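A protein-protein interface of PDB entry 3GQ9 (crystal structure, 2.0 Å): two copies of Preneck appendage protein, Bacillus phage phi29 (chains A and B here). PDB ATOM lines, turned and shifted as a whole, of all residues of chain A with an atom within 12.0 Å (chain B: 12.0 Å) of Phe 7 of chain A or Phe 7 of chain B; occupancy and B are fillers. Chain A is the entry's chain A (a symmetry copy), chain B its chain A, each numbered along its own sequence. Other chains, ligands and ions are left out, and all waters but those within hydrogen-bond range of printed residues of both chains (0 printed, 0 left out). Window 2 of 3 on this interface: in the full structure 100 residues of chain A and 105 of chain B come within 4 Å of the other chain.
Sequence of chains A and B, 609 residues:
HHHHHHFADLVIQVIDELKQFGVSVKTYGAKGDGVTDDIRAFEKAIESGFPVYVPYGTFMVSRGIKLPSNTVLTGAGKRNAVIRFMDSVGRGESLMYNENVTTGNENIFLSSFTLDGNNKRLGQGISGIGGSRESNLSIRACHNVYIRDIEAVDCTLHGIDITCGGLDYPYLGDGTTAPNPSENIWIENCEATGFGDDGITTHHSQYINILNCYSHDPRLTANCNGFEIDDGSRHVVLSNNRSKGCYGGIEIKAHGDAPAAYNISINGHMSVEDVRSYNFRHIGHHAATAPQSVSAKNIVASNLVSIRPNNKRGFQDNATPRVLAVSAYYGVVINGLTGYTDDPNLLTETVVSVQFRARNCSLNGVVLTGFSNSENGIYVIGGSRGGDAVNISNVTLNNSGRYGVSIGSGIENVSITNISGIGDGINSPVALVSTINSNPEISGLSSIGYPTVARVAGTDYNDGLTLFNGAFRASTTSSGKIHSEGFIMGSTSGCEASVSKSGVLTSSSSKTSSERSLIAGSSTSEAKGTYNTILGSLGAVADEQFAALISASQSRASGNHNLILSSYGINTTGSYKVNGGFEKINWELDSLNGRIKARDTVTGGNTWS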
ATOM      1  N   HIS A   6      32.632   0.659  26.403  1.00  0.00           N
ATOM      2  CA  HIS A   6      31.448   1.231  25.679  1.00  0.00           C
ATOM      3  C   HIS A   6      30.571   0.144  25.048  1.00  0.00           C
ATOM      4  O   HIS A   6      29.337   0.204  25.136  1.00  0.00           O
ATOM      5  CB  HIS A   6      31.895   2.224  24.607  1.00  0.00           C
ATOM      6  CG  HIS A   6      31.222   3.559  24.706  1.00  0.00           C
ATOM      7  ND1 HIS A   6      29.904   3.759  24.346  1.00  0.00           N
ATOM      8  CD2 HIS A   6      31.683   4.762  25.133  1.00  0.00           C
ATOM      9  CE1 HIS A   6      29.585   5.028  24.544  1.00  0.00           C
ATOM     10  NE2 HIS A   6      30.646   5.657  25.020  1.00  0.00           N
ATOM     11  N   PHE A   7      31.212  -0.828  24.395  1.00  0.00           N
ATOM     12  CA  PHE A   7      30.533  -2.033  23.915  1.00  0.00           C
ATOM     13  C   PHE A   7      30.016  -2.841  25.104  1.00  0.00           C
ATOM     14  O   PHE A   7      28.876  -3.296  25.101  1.00  0.00           O
ATOM     15  CB  PHE A   7      31.487  -2.874  23.058  1.00  0.00           C
ATOM     16  CG  PHE A   7      31.068  -4.318  22.885  1.00  0.00           C
ATOM     17  CD1 PHE A   7      30.013  -4.660  22.041  1.00  0.00           C
ATOM     18  CD2 PHE A   7      31.751  -5.339  23.548  1.00  0.00           C
ATOM     19  CE1 PHE A   7      29.636  -6.000  21.866  1.00  0.00           C
ATOM     20  CE2 PHE A   7      31.383  -6.674  23.385  1.00  0.00           C
ATOM     21  CZ  PHE A   7      30.321  -7.006  22.538  1.00  0.00           C
ATOM     22  N   ALA A   8      30.871  -3.006  26.112  1.00  0.00           N
ATOM     23  CA  ALA A   8      30.512  -3.676  27.354  1.00  0.00           C
ATOM     24  C   ALA A   8      29.273  -3.039  27.974  1.00  0.00           C
ATOM     25  O   ALA A   8      28.368  -3.741  28.413  1.00  0.00           O
ATOM     26  CB  ALA A   8      31.681  -3.647  28.331  1.00  0.00           C
ATOM     27  N   ASP A   9      29.234  -1.709  27.990  1.00  0.00           N
ATOM     28  CA  ASP A   9      28.060  -0.988  28.470  1.00  0.00           C
ATOM     29  C   ASP A   9      26.783  -1.387  27.722  1.00  0.00           C
ATOM     30  O   ASP A   9      25.736  -1.576  28.345  1.00  0.00           O
ATOM     31  CB  ASP A   9      28.279   0.528  28.409  1.00  0.00           C
ATOM     32  CG  ASP A   9      29.160   1.053  29.548  1.00  0.00           C
ATOM     33  OD1 ASP A   9      29.483   0.298  30.494  1.00  0.00           O
ATOM     34  OD2 ASP A   9      29.530   2.247  29.497  1.00  0.00           O
ATOM     35  N   LEU A  10      26.871  -1.531  26.399  1.00  0.00           N
ATOM     36  CA  LEU A  10      25.715  -1.945  25.600  1.00  0.00           C
ATOM     37  C   LEU A  10      25.275  -3.372  25.890  1.00  0.00           C
ATOM     38  O   LEU A  10      24.078  -3.633  25.972  1.00  0.00           O
ATOM     39  CB  LEU A  10      25.973  -1.800  24.098  1.00  0.00           C
ATOM     40  CG  LEU A  10      25.816  -0.438  23.425  1.00  0.00           C
ATOM     41  CD1 LEU A  10      25.809  -0.647  21.914  1.00  0.00           C
ATOM     42  CD2 LEU A  10      24.552   0.305  23.862  1.00  0.00           C
ATOM     43  N   VAL A  11      26.237  -4.287  26.005  1.00  0.00           N
ATOM     44  CA  VAL A  11      25.944  -5.677  26.369  1.00  0.00           C
ATOM     45  C   VAL A  11      25.224  -5.727  27.723  1.00  0.00           C
ATOM     46  O   VAL A  11      24.184  -6.370  27.854  1.00  0.00           O
ATOM     47  CB  VAL A  11      27.223  -6.551  26.394  1.00  0.00           C
ATOM     48  CG1 VAL A  11      26.912  -7.968  26.852  1.00  0.00           C
ATOM     49  CG2 VAL A  11      27.865  -6.577  25.013  1.00  0.00           C
ATOM     50  N   ILE A  12      25.775  -5.015  28.705  1.00  0.00           N
ATOM     51  CA  ILE A  12      25.182  -4.890  30.043  1.00  0.00           C
ATOM     52  C   ILE A  12      23.743  -4.370  29.996  1.00  0.00           C
ATOM     53  O   ILE A  12      22.867  -4.930  30.662  1.00  0.00           O
ATOM     54  CB  ILE A  12      26.089  -4.033  30.984  1.00  0.00           C
ATOM     55  CG1 ILE A  12      27.371  -4.807  31.320  1.00  0.00           C
ATOM     56  CG2 ILE A  12      25.354  -3.630  32.263  1.00  0.00           C
ATOM     57  CD1 ILE A  12      28.446  -3.988  32.028  1.00  0.00           C
ATOM     58  N   GLN A  13      23.492  -3.332  29.193  1.00  0.00           N
ATOM     59  CA  GLN A  13      22.129  -2.818  28.981  1.00  0.00           C
ATOM     60  C   GLN A  13      21.151  -3.897  28.512  1.00  0.00           C
ATOM     61  O   GLN A  13      20.004  -3.928  28.955  1.00  0.00           O
ATOM     62  CB  GLN A  13      22.116  -1.641  27.997  1.00  0.00           C
ATOM     63  CG  GLN A  13      22.574  -0.309  28.594  1.00  0.00           C
ATOM     64  CD  GLN A  13      22.736   0.807  27.547  1.00  0.00           C
ATOM     65  OE1 GLN A  13      21.947   0.924  26.602  1.00  0.00           O
ATOM     66  NE2 GLN A  13      23.770   1.632  27.723  1.00  0.00           N
ATOM     67  N   VAL A  14      21.605  -4.778  27.624  1.00  0.00           N
ATOM     68  CA  VAL A  14      20.789  -5.894  27.138  1.00  0.00           C
ATOM     69  C   VAL A  14      20.503  -6.863  28.291  1.00  0.00           C
ATOM     70  O   VAL A  14      19.352  -7.259  28.508  1.00  0.00           O
ATOM     71  CB  VAL A  14      21.474  -6.652  25.963  1.00  0.00           C
ATOM     72  CG1 VAL A  14      20.638  -7.858  25.522  1.00  0.00           C
ATOM     73  CG2 VAL A  14      21.715  -5.725  24.784  1.00  0.00           C
ATOM     74  N   ILE A  15      21.560  -7.210  29.026  1.00  0.00           N
ATOM     75  CA  ILE A  15      21.469  -8.087  30.199  1.00  0.00           C
ATOM     76  C   ILE A  15      20.501  -7.505  31.236  1.00  0.00           C
ATOM     77  O   ILE A  15      19.571  -8.188  31.653  1.00  0.00           O
ATOM     78  CB  ILE A  15      22.870  -8.361  30.823  1.00  0.00           C
ATOM     79  CG1 ILE A  15      23.770  -9.085  29.822  1.00  0.00           C
ATOM     80  CG2 ILE A  15      22.746  -9.198  32.098  1.00  0.00           C
ATOM     81  CD1 ILE A  15      25.259  -9.015  30.151  1.00  0.00           C
ATOM     82  N   ASP A  16      20.707  -6.244  31.619  1.00  0.00           N
ATOM     83  CA  ASP A  16      19.803  -5.546  32.535  1.00  0.00           C
ATOM     84  C   ASP A  16      18.338  -5.671  32.100  1.00  0.00           C
ATOM     85  O   ASP A  16      17.475  -6.048  32.900  1.00  0.00           O
ATOM     86  CB  ASP A  16      20.164  -4.063  32.636  1.00  0.00           C
ATOM     87  CG  ASP A  16      21.505  -3.812  33.314  1.00  0.00           C
ATOM     88  OD1 ASP A  16      22.078  -4.741  33.927  1.00  0.00           O
ATOM     89  OD2 ASP A  16      21.988  -2.656  33.228  1.00  0.00           O
ATOM     90  N   HIS B   6      33.513 -15.694  18.010  1.00  0.00           N
ATOM     91  CA  HIS B   6      34.467 -14.613  18.424  1.00  0.00           C
ATOM     92  C   HIS B   6      33.753 -13.424  19.077  1.00  0.00           C
ATOM     93  O   HIS B   6      34.214 -12.899  20.100  1.00  0.00           O
ATOM     94  CB  HIS B   6      35.294 -14.131  17.232  1.00  0.00           C
ATOM     95  CG  HIS B   6      36.772 -14.153  17.476  1.00  0.00           C
ATOM     96  ND1 HIS B   6      37.407 -13.238  18.290  1.00  0.00           N
ATOM     97  CD2 HIS B   6      37.739 -14.988  17.019  1.00  0.00           C
ATOM     98  CE1 HIS B   6      38.703 -13.505  18.320  1.00  0.00           C
ATOM     99  NE2 HIS B   6      38.930 -14.562  17.557  1.00  0.00           N
ATOM    100  N   PHE B   7      32.647 -12.992  18.468  1.00  0.00           N
ATOM    101  CA  PHE B   7      31.751 -12.004  19.073  1.00  0.00           C
ATOM    102  C   PHE B   7      31.119 -12.588  20.335  1.00  0.00           C
ATOM    103  O   PHE B   7      31.067 -11.928  21.369  1.00  0.00           O
ATOM    104  CB  PHE B   7      30.673 -11.581  18.069  1.00  0.00           C
ATOM    105  CG  PHE B   7      29.455 -10.933  18.692  1.00  0.00           C
ATOM    106  CD1 PHE B   7      29.509  -9.628  19.179  1.00  0.00           C
ATOM    107  CD2 PHE B   7      28.243 -11.623  18.765  1.00  0.00           C
ATOM    108  CE1 PHE B   7      28.375  -9.020  19.740  1.00  0.00           C
ATOM    109  CE2 PHE B   7      27.111 -11.030  19.324  1.00  0.00           C
ATOM    110  CZ  PHE B   7      27.178  -9.722  19.811  1.00  0.00           C
ATOM    111  N   ALA B   8      30.647 -13.829  20.230  1.00  0.00           N
ATOM    112  CA  ALA B   8      30.091 -14.563  21.359  1.00  0.00           C
ATOM    113  C   ALA B   8      31.080 -14.603  22.518  1.00  0.00           C
ATOM    114  O   ALA B   8      30.702 -14.383  23.664  1.00  0.00           O
ATOM    115  CB  ALA B   8      29.698 -15.973  20.933  1.00  0.00           C
ATOM    116  N   ASP B   9      32.347 -14.869  22.210  1.00  0.00           N
ATOM    117  CA  ASP B   9      33.398 -14.841  23.220  1.00  0.00           C
ATOM    118  C   ASP B   9      33.470 -13.495  23.951  1.00  0.00           C
ATOM    119  O   ASP B   9      33.616 -13.465  25.175  1.00  0.00           O
ATOM    120  CB  ASP B   9      34.758 -15.207  22.614  1.00  0.00           C
ATOM    121  CG  ASP B   9      34.923 -16.712  22.377  1.00  0.00           C
ATOM    122  OD1 ASP B   9      34.072 -17.516  22.820  1.00  0.00           O
ATOM    123  OD2 ASP B   9      35.929 -17.095  21.740  1.00  0.00           O
ATOM    124  N   LEU B  10      33.350 -12.391  23.212  1.00  0.00           N
ATOM    125  CA  LEU B  10      33.367 -11.060  23.822  1.00  0.00           C
ATOM    126  C   LEU B  10      32.158 -10.796  24.705  1.00  0.00           C
ATOM    127  O   LEU B  10      32.304 -10.221  25.779  1.00  0.00           O
ATOM    128  CB  LEU B  10      33.471  -9.948  22.775  1.00  0.00           C
ATOM    129  CG  LEU B  10      34.831  -9.581  22.184  1.00  0.00           C
ATOM    130  CD1 LEU B  10      34.687  -8.259  21.438  1.00  0.00           C
ATOM    131  CD2 LEU B  10      35.935  -9.476  23.238  1.00  0.00           C
ATOM    132  N   VAL B  11      30.973 -11.183  24.233  1.00  0.00           N
ATOM    133  CA  VAL B  11      29.745 -11.062  25.027  1.00  0.00           C
ATOM    134  C   VAL B  11      29.891 -11.840  26.343  1.00  0.00           C
ATOM    135  O   VAL B  11      29.623 -11.304  27.417  1.00  0.00           O
ATOM    136  CB  VAL B  11      28.499 -11.538  24.242  1.00  0.00           C
ATOM    137  CG1 VAL B  11      27.249 -11.482  25.108  1.00  0.00           C
ATOM    138  CG2 VAL B  11      28.308 -10.684  22.995  1.00  0.00           C
ATOM    139  N   ILE B  12      30.347 -13.086  26.239  1.00  0.00           N
ATOM    140  CA  ILE B  12      30.615 -13.948  27.396  1.00  0.00           C
ATOM    141  C   ILE B  12      31.582 -13.302  28.391  1.00  0.00           C
ATOM    142  O   ILE B  12      31.321 -13.317  29.599  1.00  0.00           O
ATOM    143  CB  ILE B  12      31.091 -15.367  26.945  1.00  0.00           C
ATOM    144  CG1 ILE B  12      29.926 -16.128  26.298  1.00  0.00           C
ATOM    145  CG2 ILE B  12      31.671 -16.165  28.114  1.00  0.00           C
ATOM    146  CD1 ILE B  12      30.320 -17.425  25.597  1.00  0.00           C
ATOM    147  N   GLN B  13      32.672 -12.712  27.892  1.00  0.00           N
ATOM    148  CA  GLN B  13      33.615 -11.963  28.740  1.00  0.00           C
ATOM    149  C   GLN B  13      32.935 -10.862  29.558  1.00  0.00           C
ATOM    150  O   GLN B  13      33.270 -10.663  30.724  1.00  0.00           O
ATOM    151  CB  GLN B  13      34.762 -11.366  27.915  1.00  0.00           C
ATOM    152  CG  GLN B  13      35.847 -12.368  27.517  1.00  0.00           C
ATOM    153  CD  GLN B  13      36.882 -11.792  26.535  1.00  0.00           C
ATOM    154  OE1 GLN B  13      37.285 -10.627  26.634  1.00  0.00           O
ATOM    155  NE2 GLN B  13      37.313 -12.620  25.582  1.00  0.00           N
ATOM    156  N   VAL B  14      31.985 -10.158  28.949  1.00  0.00           N
ATOM    157  CA  VAL B  14      31.218  -9.116  29.638  1.00  0.00           C
ATOM    158  C   VAL B  14      30.359  -9.751  30.738  1.00  0.00           C
ATOM    159  O   VAL B  14      30.358  -9.283  31.883  1.00  0.00           O
ATOM    160  CB  VAL B  14      30.317  -8.308  28.659  1.00  0.00           C
ATOM    161  CG1 VAL B  14      29.471  -7.275  29.411  1.00  0.00           C
ATOM    162  CG2 VAL B  14      31.152  -7.620  27.591  1.00  0.00           C
ATOM    163  N   ILE B  15      29.658 -10.823  30.373  1.00  0.00           N
ATOM    164  CA  ILE B  15      28.821 -11.590  31.302  1.00  0.00           C
ATOM    165  C   ILE B  15      29.654 -12.105  32.482  1.00  0.00           C
ATOM    166  O   ILE B  15      29.303 -11.859  33.631  1.00  0.00           O
ATOM    167  CB  ILE B  15      28.079 -12.756  30.581  1.00  0.00           C
ATOM    168  CG1 ILE B  15      27.133 -12.208  29.513  1.00  0.00           C
ATOM    169  CG2 ILE B  15      27.286 -13.600  31.581  1.00  0.00           C
ATOM    170  CD1 ILE B  15      26.695 -13.237  28.474  1.00  0.00           C
ATOM    171  N   ASP B  16      30.762 -12.788  32.190  1.00  0.00           N
ATOM    172  CA  ASP B  16      31.688 -13.257  33.223  1.00  0.00           C
ATOM    173  C   ASP B  16      32.069 -12.139  34.201  1.00  0.00           C
ATOM    174  O   ASP B  16      31.972 -12.310  35.420  1.00  0.00           O
ATOM    175  CB  ASP B  16      32.965 -13.824  32.598  1.00  0.00           C
ATOM    176  CG  ASP B  16      32.734 -15.111  31.816  1.00  0.00           C
ATOM    177  OD1 ASP B  16      31.649 -15.723  31.927  1.00  0.00           O
ATOM    178  OD2 ASP B  16      33.669 -15.514  31.080  1.00  0.00           O
ATOM    179  N   GLU B  17      32.492 -10.998  33.656  1.00  0.00           N
ATOM    180  CA  GLU B  17      32.943  -9.859  34.458  1.00  0.00           C
ATOM    181  C   GLU B  17      31.839  -9.298  35.355  1.00  0.00           C
ATOM    182  O   GLU B  17      32.127  -8.711  36.405  1.00  0.00           O
ATOM    183  CB  GLU B  17      33.517  -8.766  33.542  1.00  0.00           C
ATOM    184  CG  GLU B  17      34.020  -7.496  34.249  1.00  0.00           C
ATOM    185  CD  GLU B  17      35.417  -7.635  34.866  1.00  0.00           C
ATOM    186  OE1 GLU B  17      36.076  -8.690  34.683  1.00  0.00           O
ATOM    187  OE2 GLU B  17      35.861  -6.672  35.542  1.00  0.00           O
ATOM    188  N   LEU B  18      30.582  -9.484  34.951  1.00  0.00           N
ATOM    189  CA  LEU B  18      29.447  -9.033  35.757  1.00  0.00           C
ATOM    190  C   LEU B  18      29.345  -9.759  37.097  1.00  0.00           C
ATOM    191  O   LEU B  18      28.841  -9.190  38.070  1.00  0.00           O
ATOM    192  CB  LEU B  18      28.123  -9.184  35.002  1.00  0.00           C
ATOM    193  CG  LEU B  18      27.448  -7.959  34.388  1.00  0.00           C
ATOM    194  CD1 LEU B  18      26.009  -8.329  34.048  1.00  0.00           C
ATOM    195  CD2 LEU B  18      27.483  -6.727  35.311  1.00  0.00           C
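Phe 7 of chain A touches Phe 7 of chain B (CE1 to CE1, 3.9 Å).
Leu 10 of chain B touches Phe 7 of chain A.
Ala 8 of chain A touches Val 14 of chain B.
Val 11 of chain B touches Val 11 of chain A (CG1 to CG1, 3.9 Å).
Val 14 of chain B touches Val 11 of chain A (CG1 to CG1, 3.7 Å).
Ile 12 of chain A touches Val 14 of chain B (CG1 to CG1, 3.8 Å).
CG1 of Ile 15 of chain B touches CD1 of Ile 15 of chain A, at 3.8 Å.
Ile 15 of chain A touches Leu 18 of chain B.
No residue of chain B comes within 4 Å of His 6 of chain A.
Of the printed residues of chain B, Phe 7 of chain A touches Phe 7 (3.9 Å) and Leu 10 (3.9 Å).
Ala 8 of chain A touches one residue of chain B.
No residue of chain B comes within 4 Å of Leu 10 of chain A.
Of the printed residues of chain B, Val 11 of chain A touches Val 11 and Val 14.
Printed residues of chain B within 4 Å of Ile 12 of chain A: Val 14 (3.8 Å).
Of the printed residues of chain B, Ile 15 of chain A touches Ile 15 (3.8 Å) and Leu 18 (3.9 Å).
Asp 16 of chain A touches none of the printed residues of chain B.
No residue of chain A comes within 4 Å of His 6 of chain B.
Phe 7 of chain B touches one residue of chain A.
No residue of chain A comes within 4 Å of Ala 8 of chain B.
Of chain A, only Phe 7 comes within 4 Å of Leu 10 of chain B.
Of the printed residues of chain A, Ile 15 of chain B touches Ile 15.
Of the printed residues of chain A, Leu 18 of chain B touches Ile 15 (3.9 Å).
The nearest residue of chain B that does not touch Phe 7 of chain A is Val 11 of chain B (4.2 Å).
The nearest residue of chain A that does not touch Phe 7 of chain B is Val 11 of chain A (5.8 Å).
The nearest printed residue of chain B that does not touch Ile 12 of chain A is Leu 18 of chain B (4.4 Å).
Of the 11 printed residues of chain A, 5 touch a printed residue of chain B.
Printed residues of chain B that touch a printed residue of chain A: Phe 7, Leu 10, Val 11, Val 14, Ile 15 and Leu 18.
Hydrophobic or aromatic side chains of chain B that line the printed part of chain A: Phe 7, Leu 10, Val 11, Val 14, Ile 15 and Leu 18.
Phe 7 of chain A touches its own counterpart, Phe 7 of chain B.
Phe 7 of chain A touches Leu 10 of chain B, but with the chains exchanged Leu 10 of chain A does not touch Phe 7 of chain B (8.8 Å).
Ala 8 of chain A touches Val 14 of chain B, but with the chains exchanged Val 14 of chain A does not touch Ala 8 of chain B (12.1 Å).
Ile 12 of chain A touches Val 14 of chain B, but with the chains exchanged Val 14 of chain A does not touch Ile 12 of chain B (11.0 Å).
Positions printed for both chains: 6, 7, 8, 9, 10, 11, 12, 13, 14, 15 and 16.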
